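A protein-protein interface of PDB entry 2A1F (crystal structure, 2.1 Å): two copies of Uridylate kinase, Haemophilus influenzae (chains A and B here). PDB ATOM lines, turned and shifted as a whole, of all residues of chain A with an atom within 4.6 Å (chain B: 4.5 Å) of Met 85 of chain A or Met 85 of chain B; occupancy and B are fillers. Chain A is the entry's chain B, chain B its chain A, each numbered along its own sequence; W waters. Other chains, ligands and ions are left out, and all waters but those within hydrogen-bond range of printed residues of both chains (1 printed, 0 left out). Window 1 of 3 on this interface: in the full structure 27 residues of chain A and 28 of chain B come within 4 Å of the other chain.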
ATOM      1  N   LEU A  59      -0.175   9.845   5.972  1.00  0.00           N
ATOM      2  CA  LEU A  59      -0.800   9.548   7.259  1.00  0.00           C
ATOM      3  C   LEU A  59      -2.277   9.904   7.309  1.00  0.00           C
ATOM      4  O   LEU A  59      -3.033   9.282   8.062  1.00  0.00           O
ATOM      5  CB  LEU A  59      -0.093  10.315   8.365  1.00  0.00           C
ATOM      6  CG  LEU A  59       1.293   9.845   8.766  1.00  0.00           C
ATOM      7  CD1 LEU A  59       1.880  10.741   9.858  1.00  0.00           C
ATOM      8  CD2 LEU A  59       1.234   8.391   9.219  1.00  0.00           C
ATOM      9  N   PHE A  60      -2.679  10.925   6.565  1.00  0.00           N
ATOM     10  CA  PHE A  60      -4.069  11.334   6.513  1.00  0.00           C
ATOM     11  C   PHE A  60      -4.456  11.840   5.140  1.00  0.00           C
ATOM     12  O   PHE A  60      -3.897  12.805   4.642  1.00  0.00           O
ATOM     13  CB  PHE A  60      -4.386  12.442   7.542  1.00  0.00           C
ATOM     14  CG  PHE A  60      -5.835  12.873   7.522  1.00  0.00           C
ATOM     15  CD1 PHE A  60      -6.825  12.018   7.948  1.00  0.00           C
ATOM     16  CD2 PHE A  60      -6.208  14.095   7.002  1.00  0.00           C
ATOM     17  CE1 PHE A  60      -8.156  12.393   7.895  1.00  0.00           C
ATOM     18  CE2 PHE A  60      -7.531  14.468   6.951  1.00  0.00           C
ATOM     19  CZ  PHE A  60      -8.502  13.621   7.397  1.00  0.00           C
ATOM     20  N   MET A  78      -6.475  18.263  10.943  1.00  0.00           N
ATOM     21  CA  MET A  78      -5.970  16.881  11.020  1.00  0.00           C
ATOM     22  C   MET A  78      -4.681  16.704  10.185  1.00  0.00           C
ATOM     23  O   MET A  78      -3.721  16.112  10.649  1.00  0.00           O
ATOM     24  CB  MET A  78      -7.043  15.884  10.597  1.00  0.00           C
ATOM     25  CG  MET A  78      -8.208  15.772  11.609  1.00  0.00           C
ATOM     26  SD  MET A  78      -9.604  14.849  10.946  1.00  0.00           S
ATOM     27  CE  MET A  78      -9.041  13.177  11.076  1.00  0.00           C
ATOM     28  N   LEU A  81      -1.589  18.313  11.980  1.00  0.00           N
ATOM     29  CA  LEU A  81      -1.053  17.458  13.024  1.00  0.00           C
ATOM     30  C   LEU A  81      -0.238  16.300  12.450  1.00  0.00           C
ATOM     31  O   LEU A  81       0.761  15.906  13.030  1.00  0.00           O
ATOM     32  CB  LEU A  81      -2.203  16.893  13.876  1.00  0.00           C
ATOM     33  CG  LEU A  81      -3.052  17.906  14.635  1.00  0.00           C
ATOM     34  CD1 LEU A  81      -4.271  17.216  15.225  1.00  0.00           C
ATOM     35  CD2 LEU A  81      -2.213  18.523  15.726  1.00  0.00           C
ATOM     36  N   ALA A  82      -0.718  15.744  11.333  1.00  0.00           N
ATOM     37  CA  ALA A  82       0.012  14.728  10.546  1.00  0.00           C
ATOM     38  C   ALA A  82       1.386  15.220  10.098  1.00  0.00           C
ATOM     39  O   ALA A  82       2.358  14.464  10.150  1.00  0.00           O
ATOM     40  CB  ALA A  82      -0.798  14.275   9.310  1.00  0.00           C
ATOM     41  N   THR A  83       1.494  16.479   9.676  1.00  0.00           N
ATOM     42  CA  THR A  83       2.825  16.992   9.342  1.00  0.00           C
ATOM     43  C   THR A  83       3.784  17.045  10.527  1.00  0.00           C
ATOM     44  O   THR A  83       4.989  16.954  10.317  1.00  0.00           O
ATOM     45  CB  THR A  83       2.831  18.354   8.672  1.00  0.00           C
ATOM     46  OG1 THR A  83       2.395  19.370   9.591  1.00  0.00           O
ATOM     47  CG2 THR A  83       1.924  18.325   7.421  1.00  0.00           C
ATOM     48  N   VAL A  84       3.274  17.176  11.753  1.00  0.00           N
ATOM     49  CA  VAL A  84       4.142  17.196  12.957  1.00  0.00           C
ATOM     50  C   VAL A  84       4.664  15.792  13.218  1.00  0.00           C
ATOM     51  O   VAL A  84       5.836  15.605  13.579  1.00  0.00           O
ATOM     52  CB  VAL A  84       3.406  17.783  14.202  1.00  0.00           C
ATOM     53  CG1 VAL A  84       4.382  18.038  15.388  1.00  0.00           C
ATOM     54  CG2 VAL A  84       2.707  19.085  13.837  1.00  0.00           C
ATOM     55  N   MET A  85       3.789  14.788  13.037  1.00  0.00           N
ATOM     56  CA  MET A  85       4.178  13.411  13.214  1.00  0.00           C
ATOM     57  C   MET A  85       5.304  13.054  12.237  1.00  0.00           C
ATOM     58  O   MET A  85       6.270  12.408  12.609  1.00  0.00           O
ATOM     59  CB  MET A  85       2.985  12.488  12.995  1.00  0.00           C
ATOM     60  CG  MET A  85       1.868  12.644  14.042  1.00  0.00           C
ATOM     61  SD  MET A  85       0.324  11.811  13.599  1.00  0.00           S
ATOM     62  CE  MET A  85       0.890  10.124  13.531  1.00  0.00           C
ATOM     63  N   ASN A  86       5.167  13.496  10.984  1.00  0.00           N
ATOM     64  CA  ASN A  86       6.234  13.326  10.018  1.00  0.00           C
ATOM     65  C   ASN A  86       7.505  14.053  10.423  1.00  0.00           C
ATOM     66  O   ASN A  86       8.596  13.531  10.224  1.00  0.00           O
ATOM     67  CB  ASN A  86       5.797  13.775   8.612  1.00  0.00           C
ATOM     68  CG  ASN A  86       4.946  12.726   7.906  1.00  0.00           C
ATOM     69  OD1 ASN A  86       5.097  11.529   8.141  1.00  0.00           O
ATOM     70  ND2 ASN A  86       4.029  13.179   7.055  1.00  0.00           N
ATOM     71  N   GLY A  87       7.340  15.271  10.925  1.00  0.00           N
ATOM     72  CA  GLY A  87       8.444  16.063  11.420  1.00  0.00           C
ATOM     73  C   GLY A  87       9.222  15.380  12.518  1.00  0.00           C
ATOM     74  O   GLY A  87      10.454  15.485  12.559  1.00  0.00           O
ATOM     75  N   LEU A  88       8.499  14.715  13.425  1.00  0.00           N
ATOM     76  CA  LEU A  88       9.109  14.060  14.566  1.00  0.00           C
ATOM     77  C   LEU A  88       9.944  12.867  14.104  1.00  0.00           C
ATOM     78  O   LEU A  88      11.031  12.637  14.609  1.00  0.00           O
ATOM     79  CB  LEU A  88       8.025  13.622  15.594  1.00  0.00           C
ATOM     80  CG  LEU A  88       7.405  14.709  16.484  1.00  0.00           C
ATOM     81  CD1 LEU A  88       6.103  14.267  17.142  1.00  0.00           C
ATOM     82  CD2 LEU A  88       8.392  15.166  17.569  1.00  0.00           C
ATOM     83  N   ALA A  89       9.407  12.105  13.147  1.00  0.00           N
ATOM     84  CA  ALA A  89      10.096  10.963  12.572  1.00  0.00           C
ATOM     85  C   ALA A  89      11.362  11.419  11.846  1.00  0.00           C
ATOM     86  O   ALA A  89      12.402  10.821  12.027  1.00  0.00           O
ATOM     87  CB  ALA A  89       9.161  10.198  11.607  1.00  0.00           C
ATOM     88  N   LEU B  59      -3.947   5.096  13.133  1.00  0.00           N
ATOM     89  CA  LEU B  59      -3.180   6.099  12.380  1.00  0.00           C
ATOM     90  C   LEU B  59      -1.657   5.978  12.522  1.00  0.00           C
ATOM     91  O   LEU B  59      -0.916   6.384  11.623  1.00  0.00           O
ATOM     92  CB  LEU B  59      -3.592   7.503  12.815  1.00  0.00           C
ATOM     93  CG  LEU B  59      -5.001   7.981  12.500  1.00  0.00           C
ATOM     94  CD1 LEU B  59      -5.208   9.356  13.092  1.00  0.00           C
ATOM     95  CD2 LEU B  59      -5.303   7.976  10.993  1.00  0.00           C
ATOM     96  N   PHE B  60      -1.191   5.481  13.656  1.00  0.00           N
ATOM     97  CA  PHE B  60       0.225   5.291  13.872  1.00  0.00           C
ATOM     98  C   PHE B  60       0.495   4.056  14.697  1.00  0.00           C
ATOM     99  O   PHE B  60       0.014   3.935  15.827  1.00  0.00           O
ATOM    100  CB  PHE B  60       0.866   6.492  14.587  1.00  0.00           C
ATOM    101  CG  PHE B  60       2.355   6.339  14.777  1.00  0.00           C
ATOM    102  CD1 PHE B  60       3.202   6.351  13.684  1.00  0.00           C
ATOM    103  CD2 PHE B  60       2.895   6.104  16.020  1.00  0.00           C
ATOM    104  CE1 PHE B  60       4.563   6.171  13.839  1.00  0.00           C
ATOM    105  CE2 PHE B  60       4.260   5.922  16.181  1.00  0.00           C
ATOM    106  CZ  PHE B  60       5.091   5.963  15.099  1.00  0.00           C
ATOM    107  N   MET B  78       4.257  11.003  18.796  1.00  0.00           N
ATOM    108  CA  MET B  78       3.547  10.827  17.513  1.00  0.00           C
ATOM    109  C   MET B  78       2.155  10.185  17.739  1.00  0.00           C
ATOM    110  O   MET B  78       1.159  10.593  17.138  1.00  0.00           O
ATOM    111  CB  MET B  78       4.384   9.992  16.531  1.00  0.00           C
ATOM    112  CG  MET B  78       5.687  10.678  16.017  1.00  0.00           C
ATOM    113  SD  MET B  78       6.808   9.512  15.194  1.00  0.00           S
ATOM    114  CE  MET B  78       5.958   9.223  13.646  1.00  0.00           C
ATOM    115  N   LEU B  81      -0.419  12.788  19.130  1.00  0.00           N
ATOM    116  CA  LEU B  81      -0.936  13.644  18.069  1.00  0.00           C
ATOM    117  C   LEU B  81      -1.976  12.956  17.209  1.00  0.00           C
ATOM    118  O   LEU B  81      -2.940  13.583  16.813  1.00  0.00           O
ATOM    119  CB  LEU B  81       0.201  14.180  17.170  1.00  0.00           C
ATOM    120  CG  LEU B  81       1.256  15.047  17.849  1.00  0.00           C
ATOM    121  CD1 LEU B  81       2.477  15.173  16.971  1.00  0.00           C
ATOM    122  CD2 LEU B  81       0.678  16.423  18.180  1.00  0.00           C
ATOM    123  N   ALA B  82      -1.757  11.684  16.911  1.00  0.00           N
ATOM    124  CA  ALA B  82      -2.751  10.836  16.288  1.00  0.00           C
ATOM    125  C   ALA B  82      -4.052  10.719  17.101  1.00  0.00           C
ATOM    126  O   ALA B  82      -5.112  10.649  16.507  1.00  0.00           O
ATOM    127  CB  ALA B  82      -2.177   9.425  16.045  1.00  0.00           C
ATOM    128  N   THR B  83      -3.997  10.682  18.440  1.00  0.00           N
ATOM    129  CA  THR B  83      -5.262  10.690  19.206  1.00  0.00           C
ATOM    130  C   THR B  83      -6.047  11.998  19.027  1.00  0.00           C
ATOM    131  O   THR B  83      -7.267  12.012  19.125  1.00  0.00           O
ATOM    132  CB  THR B  83      -5.110  10.404  20.718  1.00  0.00           C
ATOM    133  OG1 THR B  83      -4.442  11.483  21.374  1.00  0.00           O
ATOM    134  CG2 THR B  83      -4.348   9.069  20.957  1.00  0.00           C
ATOM    135  N   VAL B  84      -5.344  13.097  18.763  1.00  0.00           N
ATOM    136  CA  VAL B  84      -6.001  14.387  18.548  1.00  0.00           C
ATOM    137  C   VAL B  84      -6.712  14.375  17.202  1.00  0.00           C
ATOM    138  O   VAL B  84      -7.794  14.935  17.082  1.00  0.00           O
ATOM    139  CB  VAL B  84      -5.028  15.600  18.670  1.00  0.00           C
ATOM    140  CG1 VAL B  84      -5.788  16.940  18.595  1.00  0.00           C
ATOM    141  CG2 VAL B  84      -4.263  15.554  19.995  1.00  0.00           C
ATOM    142  N   MET B  85      -6.097  13.745  16.195  1.00  0.00           N
ATOM    143  CA  MET B  85      -6.704  13.616  14.877  1.00  0.00           C
ATOM    144  C   MET B  85      -7.990  12.786  14.944  1.00  0.00           C
ATOM    145  O   MET B  85      -8.996  13.139  14.359  1.00  0.00           O
ATOM    146  CB  MET B  85      -5.716  12.968  13.896  1.00  0.00           C
ATOM    147  CG  MET B  85      -4.463  13.813  13.626  1.00  0.00           C
ATOM    148  SD  MET B  85      -3.133  12.958  12.756  1.00  0.00           S
ATOM    149  CE  MET B  85      -3.985  12.709  11.214  1.00  0.00           C
ATOM    150  N   ASN B  86      -7.942  11.673  15.668  1.00  0.00           N
ATOM    151  CA  ASN B  86      -9.157  10.888  15.926  1.00  0.00           C
ATOM    152  C   ASN B  86     -10.230  11.673  16.680  1.00  0.00           C
ATOM    153  O   ASN B  86     -11.408  11.559  16.382  1.00  0.00           O
ATOM    154  CB  ASN B  86      -8.816   9.613  16.698  1.00  0.00           C
ATOM    155  CG  ASN B  86      -8.236   8.542  15.812  1.00  0.00           C
ATOM    156  OD1 ASN B  86      -8.596   8.444  14.635  1.00  0.00           O
ATOM    157  ND2 ASN B  86      -7.339   7.726  16.362  1.00  0.00           N
ATOM    158  N   GLY B  87      -9.791  12.455  17.661  1.00  0.00           N
ATOM    159  CA  GLY B  87     -10.655  13.302  18.443  1.00  0.00           C
ATOM    160  C   GLY B  87     -11.382  14.329  17.604  1.00  0.00           C
ATOM    161  O   GLY B  87     -12.569  14.575  17.819  1.00  0.00           O
ATOM    162  N   LEU B  88     -10.668  14.927  16.646  1.00  0.00           N
ATOM    163  CA  LEU B  88     -11.263  15.932  15.790  1.00  0.00           C
ATOM    164  C   LEU B  88     -12.306  15.288  14.880  1.00  0.00           C
ATOM    165  O   LEU B  88     -13.349  15.859  14.667  1.00  0.00           O
ATOM    166  CB  LEU B  88     -10.180  16.660  14.968  1.00  0.00           C
ATOM    167  CG  LEU B  88      -9.242  17.670  15.666  1.00  0.00           C
ATOM    168  CD1 LEU B  88      -7.980  17.888  14.848  1.00  0.00           C
ATOM    169  CD2 LEU B  88      -9.941  19.015  15.915  1.00  0.00           C
ATOM    170  N   ALA B  89     -12.020  14.104  14.342  1.00  0.00           N
ATOM    171  CA  ALA B  89     -12.986  13.378  13.512  1.00  0.00           C
ATOM    172  C   ALA B  89     -14.232  13.005  14.321  1.00  0.00           C
ATOM    173  O   ALA B  89     -15.353  13.214  13.857  1.00  0.00           O
ATOM    174  CB  ALA B  89     -12.349  12.122  12.906  1.00  0.00           C
HETATM  175  O   HOH W   1      -2.169   7.027   9.047  1.00  0.00           O
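Among the printed residues, merely in contact across the chains: Leu 59 of chain A with Leu 59 of chain B (3.8 Å), Phe 60 of chain A with Met 85 of chain B (3.7 Å), Met 78 of chain A with Met 85 of chain B (3.3 Å), Met 78 of chain A with Leu 88 of chain B (3.9 Å), Met 78 of chain A with Ala 89 of chain B (3.9 Å), Leu 81 of chain A with Val 84 of chain B (3.7 Å), Leu 81 of chain A with Met 85 of chain B (3.8 Å), Leu 81 of chain A with Leu 88 of chain B (3.8 Å), Ala 82 of chain A with Met 85 of chain B (3.95 Å), Val 84 of chain A with Leu 81 of chain B (3.8 Å), Met 85 of chain A with Phe 60 of chain B (3.8 Å), Met 85 of chain A with Met 78 of chain B (3.4 Å), Met 85 of chain A with Leu 81 of chain B (3.9 Å), Met 85 of chain A with Ala 82 of chain B (3.9 Å), Leu 88 of chain A with Met 78 of chain B (3.8 Å), Leu 88 of chain A with Leu 81 of chain B (3.7 Å) and Ala 89 of chain A with Met 78 of chain B (3.9 Å).
Water W1 lies within hydrogen-bond range of the backbone carbonyl oxygen of Leu 59 of chain A (2.6 Å) and the backbone carbonyl oxygen of Leu 59 of chain B (2.9 Å).
The side-chain sulfur (SD) of Met 85 of chain B sits close to the side-chain sulfur (SD) of Met 85 of chain A (3.7 Å).
Met 85 of chain A touches five residues of chain B. Met 85 of chain B touches five residues of chain A. Of the printed residues of chain A, Val 84 of chain B touches Leu 81. Of the printed residues of chain A, Leu 59 of chain B touches Leu 59 (3.8 Å). Printed residues of chain B within 4 Å of Leu 81 of chain A: Val 84, Met 85 and Leu 88. Of the printed residues of chain B, Leu 88 of chain A touches Met 78 and Leu 81. The nearest printed residue of chain A that does not touch Met 85 of chain B is Leu 59 of chain A (4.8 Å). The nearest printed residue of chain B that does not touch Val 84 of chain A is Met 78 of chain B (5.5 Å).
Hydrophobic or aromatic side chains of chain A that line the printed part of chain B: Leu 59, Phe 60, Met 78, Leu 81, Val 84, Met 85, Leu 88 and Ala 89. Of the 12 printed residues of chain B, 9 touch a printed residue of chain A. Hydrophobic or aromatic side chains of chain B within 4 Å of the printed part of chain A: Leu 59, Phe 60, Met 78, Leu 81, Val 84, Met 85, Leu 88 and Ala 89. Among the printed residues, no Asp or Glu carboxylate lies within 4 Å of a Lys or Arg side-chain nitrogen of the other chain.
Leu 59 of chain A touches its own counterpart, Leu 59 of chain B. Met 78 of chain A touches Leu 88 of chain B, and with the chains exchanged Leu 88 of chain A touches Met 78 of chain B. Leu 81 of chain A touches Met 85 of chain B, and with the chains exchanged Met 85 of chain A touches Leu 81 of chain B. Ala 82 of chain A touches Met 85 of chain B, and with the chains exchanged Met 85 of chain A touches Ala 82 of chain B. 12 positions are printed for both chains. Of the 18 pairs that touch across the chains among the printed residues, 18 have their exchanged pair printed and touching as well.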
